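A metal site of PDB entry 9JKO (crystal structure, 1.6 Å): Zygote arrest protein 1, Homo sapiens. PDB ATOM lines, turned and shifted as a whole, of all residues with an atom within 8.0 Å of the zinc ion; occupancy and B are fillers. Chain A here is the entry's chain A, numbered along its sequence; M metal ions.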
ATOM      1  N   ILE A  56       7.237  30.513 -33.557  1.00  0.00           N
ATOM      2  CA  ILE A  56       7.291  29.146 -34.042  1.00  0.00           C
ATOM      3  C   ILE A  56       6.212  28.334 -33.341  1.00  0.00           C
ATOM      4  O   ILE A  56       6.077  28.408 -32.111  1.00  0.00           O
ATOM      5  CB  ILE A  56       8.688  28.561 -33.769  1.00  0.00           C
ATOM      6  CG1 ILE A  56       9.709  29.191 -34.745  1.00  0.00           C
ATOM      7  CG2 ILE A  56       8.660  27.071 -33.935  1.00  0.00           C
ATOM      8  CD1 ILE A  56      11.178  28.879 -34.366  1.00  0.00           C
ATOM      9  N   THR A  57       5.468  27.529 -34.089  1.00  0.00           N
ATOM     10  CA  THR A  57       4.643  26.548 -33.416  1.00  0.00           C
ATOM     11  C   THR A  57       5.503  25.318 -33.142  1.00  0.00           C
ATOM     12  O   THR A  57       5.984  24.655 -34.075  1.00  0.00           O
ATOM     13  CB  THR A  57       3.393  26.214 -34.198  1.00  0.00           C
ATOM     14  OG1 THR A  57       2.513  27.342 -34.109  1.00  0.00           O
ATOM     15  CG2 THR A  57       2.697  25.007 -33.550  1.00  0.00           C
ATOM     16  N   CYS A  58       5.705  25.064 -31.856  1.00  0.00           N
ATOM     17  CA  CYS A  58       6.560  23.976 -31.407  1.00  0.00           C
ATOM     18  C   CYS A  58       6.073  22.632 -31.929  1.00  0.00           C
ATOM     19  O   CYS A  58       4.906  22.274 -31.743  1.00  0.00           O
ATOM     20  CB  CYS A  58       6.607  23.960 -29.886  1.00  0.00           C
ATOM     21  SG  CYS A  58       7.726  22.781 -29.147  1.00  0.00           S
ATOM     22  N   GLN A  59       6.978  21.870 -32.546  1.00  0.00           N
ATOM     23  CA  GLN A  59       6.596  20.539 -33.004  1.00  0.00           C
ATOM     24  C   GLN A  59       6.732  19.503 -31.913  1.00  0.00           C
ATOM     25  O   GLN A  59       6.400  18.338 -32.145  1.00  0.00           O
ATOM     26  CB  GLN A  59       7.420  20.143 -34.219  1.00  0.00           C
ATOM     27  CG  GLN A  59       7.140  21.048 -35.390  1.00  0.00           C
ATOM     28  CD  GLN A  59       5.656  21.121 -35.747  1.00  0.00           C
ATOM     29  OE1 GLN A  59       5.091  20.175 -36.311  1.00  0.00           O
ATOM     30  NE2 GLN A  59       5.035  22.266 -35.471  1.00  0.00           N
ATOM     31  N   SER A  60       7.215  19.888 -30.741  1.00  0.00           N
ATOM     32  CA  SER A  60       7.203  18.964 -29.608  1.00  0.00           C
ATOM     33  C   SER A  60       5.866  19.019 -28.867  1.00  0.00           C
ATOM     34  O   SER A  60       5.241  17.980 -28.626  1.00  0.00           O
ATOM     35  CB  SER A  60       8.372  19.286 -28.667  1.00  0.00           C
ATOM     36  OG  SER A  60       8.658  18.162 -27.854  1.00  0.00           O
ATOM     37  N   CYS A  61       5.387  20.222 -28.548  1.00  0.00           N
ATOM     38  CA  CYS A  61       4.232  20.393 -27.678  1.00  0.00           C
ATOM     39  C   CYS A  61       3.066  21.126 -28.328  1.00  0.00           C
ATOM     40  O   CYS A  61       2.034  21.317 -27.682  1.00  0.00           O
ATOM     41  CB  CYS A  61       4.631  21.174 -26.416  1.00  0.00           C
ATOM     42  SG  CYS A  61       4.799  22.942 -26.681  1.00  0.00           S
ATOM     43  N   LYS A  62       3.227  21.607 -29.570  1.00  0.00           N
ATOM     44  CA  LYS A  62       2.162  22.281 -30.302  1.00  0.00           C
ATOM     45  C   LYS A  62       1.741  23.625 -29.694  1.00  0.00           C
ATOM     46  O   LYS A  62       0.619  24.094 -29.929  1.00  0.00           O
ATOM     47  CB  LYS A  62       0.923  21.376 -30.431  1.00  0.00           C
ATOM     48  CG  LYS A  62       1.120  20.098 -31.247  1.00  0.00           C
ATOM     49  CD  LYS A  62       2.229  20.203 -32.294  1.00  0.00           C
ATOM     50  CE  LYS A  62       2.807  18.810 -32.622  1.00  0.00           C
ATOM     51  NZ  LYS A  62       1.798  17.867 -33.232  1.00  0.00           N
ATOM     52  N   GLN A  63       2.597  24.292 -28.911  1.00  0.00           N
ATOM     53  CA  GLN A  63       2.291  25.638 -28.451  1.00  0.00           C
ATOM     54  C   GLN A  63       3.304  26.671 -28.920  1.00  0.00           C
ATOM     55  O   GLN A  63       4.425  26.355 -29.335  1.00  0.00           O
ATOM     56  CB  GLN A  63       2.171  25.701 -26.943  1.00  0.00           C
ATOM     57  CG  GLN A  63       1.428  24.524 -26.340  1.00  0.00           C
ATOM     58  CD  GLN A  63       0.218  25.064 -25.660  1.00  0.00           C
ATOM     59  OE1 GLN A  63      -0.011  26.283 -25.682  1.00  0.00           O
ATOM     60  NE2 GLN A  63      -0.608  24.180 -25.099  1.00  0.00           N
ATOM     61  N   THR A  64       2.870  27.938 -28.894  1.00  0.00           N
ATOM     62  CA  THR A  64       3.795  29.054 -29.032  1.00  0.00           C
ATOM     63  C   THR A  64       4.251  29.507 -27.637  1.00  0.00           C
ATOM     64  O   THR A  64       3.563  29.284 -26.637  1.00  0.00           O
ATOM     65  CB  THR A  64       3.177  30.223 -29.812  1.00  0.00           C
ATOM     66  OG1 THR A  64       1.951  30.650 -29.202  1.00  0.00           O
ATOM     67  CG2 THR A  64       2.886  29.792 -31.247  1.00  0.00           C
ATOM     68  N   ARG A  65       5.452  30.099 -27.593  1.00  0.00           N
ATOM     69  CA  ARG A  65       6.032  30.620 -26.346  1.00  0.00           C
ATOM     70  C   ARG A  65       6.194  29.529 -25.284  1.00  0.00           C
ATOM     71  O   ARG A  65       6.091  29.800 -24.089  1.00  0.00           O
ATOM     72  CB  ARG A  65       5.217  31.794 -25.790  1.00  0.00           C
ATOM     73  N   CYS A  66       6.483  28.306 -25.715  1.00  0.00           N
ATOM     74  CA  CYS A  66       6.623  27.198 -24.748  1.00  0.00           C
ATOM     75  C   CYS A  66       8.034  27.172 -24.167  1.00  0.00           C
ATOM     76  O   CYS A  66       8.896  27.996 -24.485  1.00  0.00           O
ATOM     77  CB  CYS A  66       6.287  25.886 -25.435  1.00  0.00           C
ATOM     78  SG  CYS A  66       7.671  25.383 -26.532  1.00  0.00           S
ATOM     79  N   SER A  67       8.284  26.228 -23.242  1.00  0.00           N
ATOM     80  CA  SER A  67       9.610  26.130 -22.654  1.00  0.00           C
ATOM     81  C   SER A  67      10.364  24.877 -23.112  1.00  0.00           C
ATOM     82  O   SER A  67      11.276  24.413 -22.407  1.00  0.00           O
ATOM     83  CB  SER A  67       9.548  26.140 -21.125  1.00  0.00           C
ATOM     84  OG  SER A  67       8.589  25.222 -20.667  1.00  0.00           O
ATOM     85  N   CYS A  68       9.971  24.292 -24.238  1.00  0.00           N
ATOM     86  CA  CYS A  68      10.656  23.100 -24.718  1.00  0.00           C
ATOM     87  C   CYS A  68      12.080  23.440 -25.150  1.00  0.00           C
ATOM     88  O   CYS A  68      12.335  24.519 -25.659  1.00  0.00           O
ATOM     89  CB  CYS A  68       9.922  22.483 -25.902  1.00  0.00           C
ATOM     90  SG  CYS A  68       8.235  21.891 -25.472  1.00  0.00           S
ATOM     91  N   PRO A  69      13.028  22.523 -24.964  1.00  0.00           N
ATOM     92  CA  PRO A  69      14.397  22.828 -25.369  1.00  0.00           C
ATOM     93  C   PRO A  69      14.567  22.914 -26.874  1.00  0.00           C
ATOM     94  O   PRO A  69      15.441  23.667 -27.337  1.00  0.00           O
ATOM     95  CB  PRO A  69      15.204  21.672 -24.766  1.00  0.00           C
ATOM     96  CG  PRO A  69      14.249  20.528 -24.713  1.00  0.00           C
ATOM     97  CD  PRO A  69      12.907  21.196 -24.344  1.00  0.00           C
ATOM     98  N   VAL A  70      13.802  22.140 -27.642  1.00  0.00           N
ATOM     99  CA  VAL A  70      13.939  22.109 -29.096  1.00  0.00           C
ATOM    100  C   VAL A  70      12.529  22.176 -29.691  1.00  0.00           C
ATOM    101  O   VAL A  70      11.712  21.284 -29.437  1.00  0.00           O
ATOM    102  CB  VAL A  70      14.674  20.850 -29.574  1.00  0.00           C
ATOM    103  CG1 VAL A  70      14.670  20.786 -31.111  1.00  0.00           C
ATOM    104  CG2 VAL A  70      16.138  20.800 -29.018  1.00  0.00           C
ATOM    105  N   LYS A  71      12.254  23.212 -30.476  1.00  0.00           N
ATOM    106  CA  LYS A  71      10.929  23.393 -31.062  1.00  0.00           C
ATOM    107  C   LYS A  71      10.837  22.791 -32.447  1.00  0.00           C
ATOM    108  O   LYS A  71       9.759  22.422 -32.906  1.00  0.00           O
ATOM    109  CB  LYS A  71      10.579  24.884 -31.143  1.00  0.00           C
ATOM    110  CG  LYS A  71      10.364  25.553 -29.768  1.00  0.00           C
ATOM    111  CD  LYS A  71       9.825  26.991 -29.900  1.00  0.00           C
ATOM    112  CE  LYS A  71       9.902  27.716 -28.529  1.00  0.00           C
ATOM    113  NZ  LYS A  71       9.404  29.122 -28.712  1.00  0.00           N
ATOM    114  N   LEU A  72      11.961  22.743 -33.149  1.00  0.00           N
ATOM    115  CA  LEU A  72      12.072  22.257 -34.519  1.00  0.00           C
ATOM    116  C   LEU A  72      13.364  21.446 -34.604  1.00  0.00           C
ATOM    117  O   LEU A  72      14.414  21.945 -34.159  1.00  0.00           O
ATOM    118  CB  LEU A  72      12.152  23.421 -35.510  1.00  0.00           C
ATOM    119  CG  LEU A  72      10.913  24.331 -35.615  1.00  0.00           C
ATOM    120  CD1 LEU A  72      11.229  25.551 -36.502  1.00  0.00           C
ATOM    121  CD2 LEU A  72       9.725  23.561 -36.162  1.00  0.00           C
HETATM  122 ZN    ZN M   1       7.065  23.189 -26.965  1.00  0.00          ZN
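SG of Cys 61 sits close to N of Gln 63, at 3.4 Å.
The backbone NH of Ser 60 lies close to the side-chain sulfur of Cys 58 (3.3 Å).
N of Cys 58 lies within hydrogen-bond range of O of Gln 63, 3.1 Å away.
Within 4 Å of the zinc ion: Cys 58, Cys 61, Cys 66 and Cys 68.
The nearest printed residue that does not touch the zinc ion is Ser 60 (4.5 Å).
SG of Cys 61 is bound to the zinc ion, 2.3 Å away.
The zinc ion is bound by SG of Cys 68 (2.3 Å).
The side-chain sulfur (SG) of Cys 58 is bound to the zinc ion (2.3 Å).
SG of Cys 66 is bound to the zinc ion (2.3 Å).
The zinc ion has four donor atoms within binding distance.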
